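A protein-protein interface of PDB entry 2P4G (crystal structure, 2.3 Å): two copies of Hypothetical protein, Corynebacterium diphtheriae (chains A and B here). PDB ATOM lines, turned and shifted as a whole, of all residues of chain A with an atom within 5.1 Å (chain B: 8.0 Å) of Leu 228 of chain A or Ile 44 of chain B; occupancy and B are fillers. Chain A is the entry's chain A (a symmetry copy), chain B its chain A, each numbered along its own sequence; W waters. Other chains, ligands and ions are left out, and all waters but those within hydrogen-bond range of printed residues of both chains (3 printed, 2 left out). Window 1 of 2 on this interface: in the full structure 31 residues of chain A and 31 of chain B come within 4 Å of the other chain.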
ATOM      1  N   ALA A  40       9.816 -34.456  -7.843  1.00  0.00           N
ATOM      2  CA  ALA A  40       9.888 -33.762  -9.125  1.00  0.00           C
ATOM      3  C   ALA A  40      11.240 -33.990  -9.804  1.00  0.00           C
ATOM      4  O   ALA A  40      12.211 -34.396  -9.156  1.00  0.00           O
ATOM      5  CB  ALA A  40       9.553 -32.247  -8.948  1.00  0.00           C
ATOM      6  N   ILE A  41      11.248 -33.810 -11.122  1.00  0.00           N
ATOM      7  CA  ILE A  41      12.450 -33.865 -11.941  1.00  0.00           C
ATOM      8  C   ILE A  41      12.582 -32.556 -12.725  1.00  0.00           C
ATOM      9  O   ILE A  41      11.597 -31.966 -13.151  1.00  0.00           O
ATOM     10  CB  ILE A  41      12.437 -35.135 -12.889  1.00  0.00           C
ATOM     11  CG1 ILE A  41      13.792 -35.314 -13.591  1.00  0.00           C
ATOM     12  CG2 ILE A  41      11.313 -35.067 -13.876  1.00  0.00           C
ATOM     13  CD1 ILE A  41      13.982 -36.708 -14.181  1.00  0.00           C
ATOM     14  N   THR A  42      13.809 -32.096 -12.916  1.00  0.00           N
ATOM     15  CA  THR A  42      14.053 -30.839 -13.608  1.00  0.00           C
ATOM     16  C   THR A  42      15.370 -30.916 -14.369  1.00  0.00           C
ATOM     17  O   THR A  42      16.286 -31.632 -13.963  1.00  0.00           O
ATOM     18  CB  THR A  42      14.116 -29.651 -12.585  1.00  0.00           C
ATOM     19  OG1 THR A  42      14.292 -28.416 -13.286  1.00  0.00           O
ATOM     20  CG2 THR A  42      15.256 -29.840 -11.550  1.00  0.00           C
ATOM     21  N   GLY A  46      15.850 -25.643 -14.793  1.00  0.00           N
ATOM     22  CA  GLY A  46      14.492 -25.497 -14.277  1.00  0.00           C
ATOM     23  C   GLY A  46      13.317 -25.833 -15.164  1.00  0.00           C
ATOM     24  O   GLY A  46      12.191 -25.412 -14.874  1.00  0.00           O
ATOM     25  N   SER A  47      13.548 -26.590 -16.235  1.00  0.00           N
ATOM     26  CA  SER A  47      12.446 -27.147 -17.020  1.00  0.00           C
ATOM     27  C   SER A  47      12.044 -28.523 -16.479  1.00  0.00           C
ATOM     28  O   SER A  47      12.900 -29.368 -16.287  1.00  0.00           O
ATOM     29  CB  SER A  47      12.807 -27.246 -18.486  1.00  0.00           C
ATOM     30  OG  SER A  47      11.688 -27.726 -19.214  1.00  0.00           O
ATOM     31  N   ALA A  48      10.747 -28.723 -16.214  1.00  0.00           N
ATOM     32  CA  ALA A  48      10.215 -30.015 -15.770  1.00  0.00           C
ATOM     33  C   ALA A  48      10.071 -31.015 -16.929  1.00  0.00           C
ATOM     34  O   ALA A  48       9.903 -32.226 -16.696  1.00  0.00           O
ATOM     35  CB  ALA A  48       8.836 -29.825 -15.069  1.00  0.00           C
ATOM     36  N   PRO A 197       3.735 -29.054 -12.465  1.00  0.00           N
ATOM     37  CA  PRO A 197       4.263 -27.754 -12.005  1.00  0.00           C
ATOM     38  C   PRO A 197       3.232 -26.861 -11.314  1.00  0.00           C
ATOM     39  O   PRO A 197       3.524 -26.253 -10.277  1.00  0.00           O
ATOM     40  CB  PRO A 197       4.736 -27.096 -13.306  1.00  0.00           C
ATOM     41  CG  PRO A 197       5.141 -28.231 -14.165  1.00  0.00           C
ATOM     42  CD  PRO A 197       4.313 -29.439 -13.771  1.00  0.00           C
ATOM     43  N   TYR A 200       2.499 -28.476  -7.926  1.00  0.00           N
ATOM     44  CA  TYR A 200       3.612 -28.087  -7.044  1.00  0.00           C
ATOM     45  C   TYR A 200       3.421 -26.671  -6.555  1.00  0.00           C
ATOM     46  O   TYR A 200       3.523 -26.389  -5.365  1.00  0.00           O
ATOM     47  CB  TYR A 200       4.952 -28.128  -7.779  1.00  0.00           C
ATOM     48  CG  TYR A 200       5.392 -29.472  -8.296  1.00  0.00           C
ATOM     49  CD1 TYR A 200       5.223 -30.625  -7.552  1.00  0.00           C
ATOM     50  CD2 TYR A 200       6.054 -29.577  -9.498  1.00  0.00           C
ATOM     51  CE1 TYR A 200       5.654 -31.838  -8.018  1.00  0.00           C
ATOM     52  CE2 TYR A 200       6.475 -30.801  -9.969  1.00  0.00           C
ATOM     53  CZ  TYR A 200       6.267 -31.920  -9.232  1.00  0.00           C
ATOM     54  OH  TYR A 200       6.700 -33.148  -9.706  1.00  0.00           O
ATOM     55  N   LEU A 212      10.659 -32.068  -0.192  1.00  0.00           N
ATOM     56  CA  LEU A 212      10.753 -32.146  -1.631  1.00  0.00           C
ATOM     57  C   LEU A 212      11.835 -33.148  -1.997  1.00  0.00           C
ATOM     58  O   LEU A 212      12.942 -33.062  -1.485  1.00  0.00           O
ATOM     59  CB  LEU A 212      11.115 -30.761  -2.175  1.00  0.00           C
ATOM     60  CG  LEU A 212      11.389 -30.573  -3.659  1.00  0.00           C
ATOM     61  CD1 LEU A 212      10.198 -30.993  -4.499  1.00  0.00           C
ATOM     62  CD2 LEU A 212      11.756 -29.121  -3.865  1.00  0.00           C
ATOM     63  N   LEU A 214      13.813 -33.831  -5.242  1.00  0.00           N
ATOM     64  CA  LEU A 214      14.084 -33.206  -6.538  1.00  0.00           C
ATOM     65  C   LEU A 214      15.252 -33.929  -7.172  1.00  0.00           C
ATOM     66  O   LEU A 214      16.312 -34.105  -6.546  1.00  0.00           O
ATOM     67  CB  LEU A 214      14.392 -31.720  -6.381  1.00  0.00           C
ATOM     68  CG  LEU A 214      14.718 -30.937  -7.667  1.00  0.00           C
ATOM     69  CD1 LEU A 214      13.479 -30.736  -8.505  1.00  0.00           C
ATOM     70  CD2 LEU A 214      15.367 -29.597  -7.317  1.00  0.00           C
ATOM     71  N   SER A 226       8.822 -25.908 -19.557  1.00  0.00           N
ATOM     72  CA  SER A 226       7.858 -25.908 -18.521  1.00  0.00           C
ATOM     73  C   SER A 226       8.520 -25.577 -17.178  1.00  0.00           C
ATOM     74  O   SER A 226       9.088 -26.441 -16.499  1.00  0.00           O
ATOM     75  CB  SER A 226       7.159 -27.257 -18.515  1.00  0.00           C
ATOM     76  OG  SER A 226       6.044 -27.186 -17.657  1.00  0.00           O
ATOM     77  N   PRO A 227       8.422 -24.309 -16.776  1.00  0.00           N
ATOM     78  CA  PRO A 227       8.975 -23.924 -15.489  1.00  0.00           C
ATOM     79  C   PRO A 227       8.572 -24.920 -14.406  1.00  0.00           C
ATOM     80  O   PRO A 227       7.389 -25.237 -14.259  1.00  0.00           O
ATOM     81  CB  PRO A 227       8.358 -22.555 -15.241  1.00  0.00           C
ATOM     82  CG  PRO A 227       8.137 -22.016 -16.585  1.00  0.00           C
ATOM     83  CD  PRO A 227       7.778 -23.177 -17.461  1.00  0.00           C
ATOM     84  N   LEU A 228       9.568 -25.418 -13.682  1.00  0.00           N
ATOM     85  CA  LEU A 228       9.389 -26.421 -12.667  1.00  0.00           C
ATOM     86  C   LEU A 228       8.191 -26.146 -11.752  1.00  0.00           C
ATOM     87  O   LEU A 228       7.431 -27.064 -11.450  1.00  0.00           O
ATOM     88  CB  LEU A 228      10.667 -26.527 -11.834  1.00  0.00           C
ATOM     89  CG  LEU A 228      10.733 -27.545 -10.698  1.00  0.00           C
ATOM     90  CD1 LEU A 228      10.399 -28.960 -11.242  1.00  0.00           C
ATOM     91  CD2 LEU A 228      12.104 -27.467 -10.037  1.00  0.00           C
ATOM     92  N   PHE A 229       8.040 -24.906 -11.293  1.00  0.00           N
ATOM     93  CA  PHE A 229       6.984 -24.579 -10.353  1.00  0.00           C
ATOM     94  C   PHE A 229       5.922 -23.661 -10.939  1.00  0.00           C
ATOM     95  O   PHE A 229       5.263 -22.911 -10.219  1.00  0.00           O
ATOM     96  CB  PHE A 229       7.582 -24.023  -9.058  1.00  0.00           C
ATOM     97  CG  PHE A 229       8.415 -25.025  -8.317  1.00  0.00           C
ATOM     98  CD1 PHE A 229       7.993 -26.346  -8.193  1.00  0.00           C
ATOM     99  CD2 PHE A 229       9.618 -24.668  -7.764  1.00  0.00           C
ATOM    100  CE1 PHE A 229       8.761 -27.274  -7.516  1.00  0.00           C
ATOM    101  CE2 PHE A 229      10.391 -25.584  -7.106  1.00  0.00           C
ATOM    102  CZ  PHE A 229       9.967 -26.896  -6.971  1.00  0.00           C
ATOM    103  N   GLY A 230       5.740 -23.762 -12.249  1.00  0.00           N
ATOM    104  CA  GLY A 230       4.619 -23.127 -12.924  1.00  0.00           C
ATOM    105  C   GLY A 230       4.909 -21.740 -13.406  1.00  0.00           C
ATOM    106  O   GLY A 230       5.752 -21.039 -12.863  1.00  0.00           O
ATOM    107  N   LEU A 241      15.094 -23.784   1.723  1.00  0.00           N
ATOM    108  CA  LEU A 241      15.090 -25.220   1.869  1.00  0.00           C
ATOM    109  C   LEU A 241      16.259 -25.587   2.738  1.00  0.00           C
ATOM    110  O   LEU A 241      17.217 -24.811   2.840  1.00  0.00           O
ATOM    111  CB  LEU A 241      15.241 -25.860   0.500  1.00  0.00           C
ATOM    112  CG  LEU A 241      14.161 -25.544  -0.541  1.00  0.00           C
ATOM    113  CD1 LEU A 241      14.492 -26.173  -1.920  1.00  0.00           C
ATOM    114  CD2 LEU A 241      12.800 -26.035  -0.037  1.00  0.00           C
ATOM    115  N   TYR A 258      15.038 -32.167   0.284  1.00  0.00           N
ATOM    116  CA  TYR A 258      14.989 -30.937   1.077  1.00  0.00           C
ATOM    117  C   TYR A 258      13.796 -30.905   2.008  1.00  0.00           C
ATOM    118  O   TYR A 258      12.718 -31.396   1.673  1.00  0.00           O
ATOM    119  CB  TYR A 258      14.805 -29.733   0.175  1.00  0.00           C
ATOM    120  CG  TYR A 258      15.912 -29.459  -0.807  1.00  0.00           C
ATOM    121  CD1 TYR A 258      17.009 -28.655  -0.450  1.00  0.00           C
ATOM    122  CD2 TYR A 258      15.843 -29.948  -2.118  1.00  0.00           C
ATOM    123  CE1 TYR A 258      18.023 -28.354  -1.371  1.00  0.00           C
ATOM    124  CE2 TYR A 258      16.860 -29.664  -3.050  1.00  0.00           C
ATOM    125  CZ  TYR A 258      17.932 -28.857  -2.670  1.00  0.00           C
ATOM    126  OH  TYR A 258      18.914 -28.583  -3.579  1.00  0.00           O
ATOM    127  N   ILE B  41      25.341 -19.847 -10.434  1.00  0.00           N
ATOM    128  CA  ILE B  41      24.508 -20.181  -9.287  1.00  0.00           C
ATOM    129  C   ILE B  41      23.035 -20.078  -9.692  1.00  0.00           C
ATOM    130  O   ILE B  41      22.649 -19.224 -10.480  1.00  0.00           O
ATOM    131  CB  ILE B  41      24.856 -19.265  -8.043  1.00  0.00           C
ATOM    132  CG1 ILE B  41      24.139 -19.756  -6.777  1.00  0.00           C
ATOM    133  CG2 ILE B  41      24.550 -17.825  -8.323  1.00  0.00           C
ATOM    134  CD1 ILE B  41      24.733 -19.189  -5.492  1.00  0.00           C
ATOM    135  N   THR B  42      22.204 -20.955  -9.150  1.00  0.00           N
ATOM    136  CA  THR B  42      20.790 -20.980  -9.494  1.00  0.00           C
ATOM    137  C   THR B  42      19.974 -21.431  -8.289  1.00  0.00           C
ATOM    138  O   THR B  42      20.461 -22.192  -7.453  1.00  0.00           O
ATOM    139  CB  THR B  42      20.532 -21.963 -10.689  1.00  0.00           C
ATOM    140  OG1 THR B  42      19.150 -21.928 -11.056  1.00  0.00           O
ATOM    141  CG2 THR B  42      20.952 -23.416 -10.343  1.00  0.00           C
ATOM    142  N   SER B  43      18.741 -20.939  -8.195  1.00  0.00           N
ATOM    143  CA  SER B  43      17.741 -21.561  -7.345  1.00  0.00           C
ATOM    144  C   SER B  43      17.457 -22.951  -7.900  1.00  0.00           C
ATOM    145  O   SER B  43      17.842 -23.275  -9.037  1.00  0.00           O
ATOM    146  CB  SER B  43      16.490 -20.701  -7.310  1.00  0.00           C
ATOM    147  OG  SER B  43      15.793 -20.722  -8.534  1.00  0.00           O
ATOM    148  N   ILE B  44      16.802 -23.793  -7.112  1.00  0.00           N
ATOM    149  CA  ILE B  44      16.481 -25.138  -7.576  1.00  0.00           C
ATOM    150  C   ILE B  44      15.536 -25.142  -8.794  1.00  0.00           C
ATOM    151  O   ILE B  44      15.522 -26.090  -9.595  1.00  0.00           O
ATOM    152  CB  ILE B  44      15.909 -26.041  -6.460  1.00  0.00           C
ATOM    153  CG1 ILE B  44      14.558 -25.526  -5.944  1.00  0.00           C
ATOM    154  CG2 ILE B  44      16.953 -26.211  -5.339  1.00  0.00           C
ATOM    155  CD1 ILE B  44      13.580 -26.623  -5.537  1.00  0.00           C
ATOM    156  N   ASN B  45      14.768 -24.071  -8.937  1.00  0.00           N
ATOM    157  CA  ASN B  45      13.886 -23.917 -10.067  1.00  0.00           C
ATOM    158  C   ASN B  45      14.424 -22.993 -11.179  1.00  0.00           C
ATOM    159  O   ASN B  45      13.667 -22.528 -12.007  1.00  0.00           O
ATOM    160  CB  ASN B  45      12.480 -23.521  -9.571  1.00  0.00           C
ATOM    161  CG  ASN B  45      12.423 -22.129  -9.002  1.00  0.00           C
ATOM    162  OD1 ASN B  45      13.303 -21.689  -8.243  1.00  0.00           O
ATOM    163  ND2 ASN B  45      11.392 -21.409  -9.394  1.00  0.00           N
ATOM    164  N   GLY B  46      15.728 -22.738 -11.200  1.00  0.00           N
ATOM    165  CA  GLY B  46      16.356 -22.116 -12.362  1.00  0.00           C
ATOM    166  C   GLY B  46      16.420 -20.610 -12.459  1.00  0.00           C
ATOM    167  O   GLY B  46      16.640 -20.076 -13.553  1.00  0.00           O
ATOM    168  N   SER B  47      16.244 -19.911 -11.339  1.00  0.00           N
ATOM    169  CA  SER B  47      16.509 -18.473 -11.296  1.00  0.00           C
ATOM    170  C   SER B  47      17.967 -18.208 -10.902  1.00  0.00           C
ATOM    171  O   SER B  47      18.435 -18.758  -9.922  1.00  0.00           O
ATOM    172  CB  SER B  47      15.573 -17.768 -10.338  1.00  0.00           C
ATOM    173  OG  SER B  47      15.822 -16.372 -10.382  1.00  0.00           O
ATOM    174  N   MET B  57      22.333 -15.694  -2.694  1.00  0.00           N
ATOM    175  CA  MET B  57      22.128 -17.127  -2.762  1.00  0.00           C
ATOM    176  C   MET B  57      23.376 -17.906  -2.369  1.00  0.00           C
ATOM    177  O   MET B  57      23.274 -19.017  -1.880  1.00  0.00           O
ATOM    178  CB  MET B  57      21.644 -17.535  -4.143  1.00  0.00           C
ATOM    179  CG  MET B  57      20.171 -17.307  -4.300  1.00  0.00           C
ATOM    180  SD  MET B  57      19.471 -18.229  -5.804  1.00  0.00           S
ATOM    181  CE  MET B  57      20.341 -17.028  -7.145  1.00  0.00           C
ATOM    182  N   THR B 215      26.275 -24.212  -8.998  1.00  0.00           N
ATOM    183  CA  THR B 215      25.866 -24.270  -7.616  1.00  0.00           C
ATOM    184  C   THR B 215      24.350 -24.159  -7.582  1.00  0.00           C
ATOM    185  O   THR B 215      23.791 -23.245  -8.175  1.00  0.00           O
ATOM    186  CB  THR B 215      26.449 -23.091  -6.824  1.00  0.00           C
ATOM    187  OG1 THR B 215      27.873 -23.113  -6.956  1.00  0.00           O
ATOM    188  CG2 THR B 215      26.022 -23.143  -5.323  1.00  0.00           C
ATOM    189  N   ILE B 216      23.699 -25.088  -6.883  1.00  0.00           N
ATOM    190  CA  ILE B 216      22.243 -25.090  -6.733  1.00  0.00           C
ATOM    191  C   ILE B 216      21.919 -24.758  -5.293  1.00  0.00           C
ATOM    192  O   ILE B 216      22.254 -25.515  -4.362  1.00  0.00           O
ATOM    193  CB  ILE B 216      21.634 -26.427  -7.104  1.00  0.00           C
ATOM    194  CG1 ILE B 216      22.081 -26.806  -8.525  1.00  0.00           C
ATOM    195  CG2 ILE B 216      20.096 -26.349  -6.978  1.00  0.00           C
ATOM    196  CD1 ILE B 216      22.162 -28.258  -8.780  1.00  0.00           C
ATOM    197  N   ALA B 217      21.279 -23.605  -5.135  1.00  0.00           N
ATOM    198  CA  ALA B 217      21.070 -22.986  -3.851  1.00  0.00           C
ATOM    199  C   ALA B 217      19.761 -23.491  -3.298  1.00  0.00           C
ATOM    200  O   ALA B 217      18.799 -23.712  -4.046  1.00  0.00           O
ATOM    201  CB  ALA B 217      21.052 -21.465  -3.988  1.00  0.00           C
ATOM    202  N   PRO B 218      19.718 -23.713  -1.971  1.00  0.00           N
ATOM    203  CA  PRO B 218      18.539 -24.285  -1.353  1.00  0.00           C
ATOM    204  C   PRO B 218      17.385 -23.275  -1.294  1.00  0.00           C
ATOM    205  O   PRO B 218      16.892 -22.943  -0.216  1.00  0.00           O
ATOM    206  CB  PRO B 218      19.049 -24.643   0.041  1.00  0.00           C
ATOM    207  CG  PRO B 218      20.072 -23.577   0.331  1.00  0.00           C
ATOM    208  CD  PRO B 218      20.771 -23.410  -0.975  1.00  0.00           C
ATOM    209  N   ASN B 219      16.959 -22.766  -2.441  1.00  0.00           N
ATOM    210  CA  ASN B 219      15.776 -21.917  -2.468  1.00  0.00           C
ATOM    211  C   ASN B 219      14.915 -22.036  -3.719  1.00  0.00           C
ATOM    212  O   ASN B 219      15.349 -22.524  -4.757  1.00  0.00           O
ATOM    213  CB  ASN B 219      16.106 -20.457  -2.118  1.00  0.00           C
ATOM    214  CG  ASN B 219      17.374 -19.974  -2.739  1.00  0.00           C
ATOM    215  OD1 ASN B 219      18.363 -19.682  -2.044  1.00  0.00           O
ATOM    216  ND2 ASN B 219      17.369 -19.891  -4.060  1.00  0.00           N
ATOM    217  N   ILE B 220      13.654 -21.656  -3.557  1.00  0.00           N
ATOM    218  CA  ILE B 220      12.658 -21.648  -4.626  1.00  0.00           C
ATOM    219  C   ILE B 220      12.288 -20.208  -4.863  1.00  0.00           C
ATOM    220  O   ILE B 220      11.995 -19.514  -3.930  1.00  0.00           O
ATOM    221  CB  ILE B 220      11.377 -22.365  -4.207  1.00  0.00           C
ATOM    222  CG1 ILE B 220      11.664 -23.853  -3.962  1.00  0.00           C
ATOM    223  CG2 ILE B 220      10.279 -22.106  -5.225  1.00  0.00           C
ATOM    224  CD1 ILE B 220      10.457 -24.676  -3.601  1.00  0.00           C
ATOM    225  N   ILE B 221      12.320 -19.774  -6.115  1.00  0.00           N
ATOM    226  CA  ILE B 221      11.983 -18.400  -6.504  1.00  0.00           C
ATOM    227  C   ILE B 221      10.953 -18.458  -7.634  1.00  0.00           C
ATOM    228  O   ILE B 221      11.258 -18.937  -8.741  1.00  0.00           O
ATOM    229  CB  ILE B 221      13.237 -17.639  -6.970  1.00  0.00           C
ATOM    230  CG1 ILE B 221      14.289 -17.621  -5.829  1.00  0.00           C
ATOM    231  CG2 ILE B 221      12.854 -16.227  -7.420  1.00  0.00           C
ATOM    232  CD1 ILE B 221      15.703 -17.205  -6.238  1.00  0.00           C
ATOM    233  N   CYS B 222       9.728 -18.031  -7.322  1.00  0.00           N
ATOM    234  CA  CYS B 222       8.619 -17.938  -8.277  1.00  0.00           C
ATOM    235  C   CYS B 222       8.041 -16.538  -8.269  1.00  0.00           C
ATOM    236  O   CYS B 222       7.655 -16.042  -7.215  1.00  0.00           O
ATOM    237  CB  CYS B 222       7.498 -18.871  -7.902  1.00  0.00           C
ATOM    238  SG  CYS B 222       8.004 -20.526  -7.928  1.00  0.00           S
ATOM    239  N   VAL B 224      10.371 -17.210 -11.747  1.00  0.00           N
ATOM    240  CA  VAL B 224      11.794 -17.175 -12.001  1.00  0.00           C
ATOM    241  C   VAL B 224      12.146 -15.728 -12.385  1.00  0.00           C
ATOM    242  O   VAL B 224      11.650 -15.200 -13.375  1.00  0.00           O
ATOM    243  CB  VAL B 224      12.194 -18.190 -13.094  1.00  0.00           C
ATOM    244  CG1 VAL B 224      13.535 -17.886 -13.621  1.00  0.00           C
ATOM    245  CG2 VAL B 224      12.155 -19.587 -12.546  1.00  0.00           C
ATOM    246  N   GLY B 252      23.822 -26.320   2.660  1.00  0.00           N
ATOM    247  CA  GLY B 252      22.945 -27.085   1.788  1.00  0.00           C
ATOM    248  C   GLY B 252      22.988 -26.663   0.336  1.00  0.00           C
ATOM    249  O   GLY B 252      22.108 -27.036  -0.445  1.00  0.00           O
ATOM    250  N   ILE B 254      24.413 -27.088  -3.328  1.00  0.00           N
ATOM    251  CA  ILE B 254      24.963 -28.235  -4.074  1.00  0.00           C
ATOM    252  C   ILE B 254      25.950 -27.632  -5.045  1.00  0.00           C
ATOM    253  O   ILE B 254      25.682 -26.590  -5.655  1.00  0.00           O
ATOM    254  CB  ILE B 254      23.907 -29.052  -4.853  1.00  0.00           C
ATOM    255  CG1 ILE B 254      22.805 -29.562  -3.929  1.00  0.00           C
ATOM    256  CG2 ILE B 254      24.545 -30.259  -5.589  1.00  0.00           C
ATOM    257  CD1 ILE B 254      21.610 -30.161  -4.716  1.00  0.00           C
HETATM  258  O   HOH W   1      20.545 -26.727  -2.675  1.00  0.00           O
HETATM  259  O   HOH W   2      11.919 -22.728 -13.741  1.00  0.00           O
HETATM  260  O   HOH W   3       7.996 -20.712 -11.677  1.00  0.00           O
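N of Leu 241 of chain A is in hydrogen-bond range of O of Pro 218 of chain B, at 2.8 Å.
Among the printed residues, pairs that only touch across the chains: Gly 46 of chain A with Asn 45 of chain B, Leu 212 of chain A with Ile 44 of chain B, Leu 214 of chain A with Ile 44 of chain B, Leu 228 of chain A with Ile 44 of chain B, Leu 228 of chain A with Asn 45 of chain B, Phe 229 of chain A with Ile 44 of chain B, Phe 229 of chain A with Asn 45 of chain B, Phe 229 of chain A with Ile 220 of chain B, Phe 229 of chain A with Cys 222 of chain B, Leu 241 of chain A with Ile 44 of chain B, Tyr 258 of chain A with Ile 44 of chain B and Tyr 258 of chain A with Ile 254 of chain B.
Printed residues of chain B that touch a printed residue of chain A: Ile 44, Asn 45, Pro 218, Ile 220, Cys 222 and Ile 254.
Of the 17 printed residues of chain A, 7 touch a printed residue of chain B.
Hydrophobic or aromatic side chains of chain A within 4 Å of the printed part of chain B: Leu 212, Leu 214, Leu 228, Phe 229, Leu 241 and Tyr 258.
Among the printed residues, 13 pairs touch across the chains.
Among the printed residues, no Asp or Glu carboxylate lies within 4 Å of a Lys or Arg side-chain nitrogen of the other chain.
Leu 228 of chain A touches two residues of chain B.
Ile 44 of chain B touches just these residues of chain A: Leu 212, Leu 214, Leu 228, Phe 229, Leu 241 and Tyr 258.
Printed residues of chain B within 4 Å of Tyr 258 of chain A: Ile 44 (3.5 Å) and Ile 254 (3.3 Å).
Of the printed residues of chain A, Asn 45 of chain B touches Gly 46 (3.8 Å), Leu 228 (3.97 Å) and Phe 229 (3.6 Å).
Of the printed residues of chain A, Ile 254 of chain B touches Tyr 258.
Gly 46 of chain B touches none of the printed residues of chain A.
Ala 40 of chain A touches none of the printed residues of chain B.
The nearest residue of chain B that does not touch Leu 228 of chain A is Gly 46 of chain B (6.1 Å).
The nearest printed residue of chain A that does not touch Ile 220 of chain B is Leu 241 of chain A (4.2 Å).
4 positions are printed for both chains.
Water W2 lies within hydrogen-bond range of O of Asn 45 of chain B and O of Gly 46 of chain A.
Water W3 bridges the backbone carbonyl oxygen of Gly 230 of chain A (2.6 Å) and the side-chain sulfur of Cys 222 of chain B (3.8 Å).
Water W1 lies within hydrogen-bond range of OH of Tyr 258 of chain A, O of Ile 216 of chain B and O of Gly 252 of chain B.
OD1 of Asn 45 of chain B lies within hydrogen-bond range of OG of Ser 43 of chain B (2.7 Å).
The backbone NH (N) of Ile 44 of chain B is in hydrogen-bond range of the backbone carbonyl oxygen (O) of Asn 219 of chain B (3.0 Å).
ND2 of Asn 45 of chain B is in hydrogen-bond range of O of Ile 221 of chain B, 2.6 Å away.
The side-chain sulfur of Cys 222 of chain B sits at hydrogen-bond distance from the side-chain amide nitrogen of Asn 45 of chain B, at 3.8 Å.
N of Ile 216 of chain B lies within hydrogen-bond range of O of Ile 254 of chain B.
N of Leu 212 of chain A sits at hydrogen-bond distance from O of Tyr 258 of chain A, at 2.9 Å.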
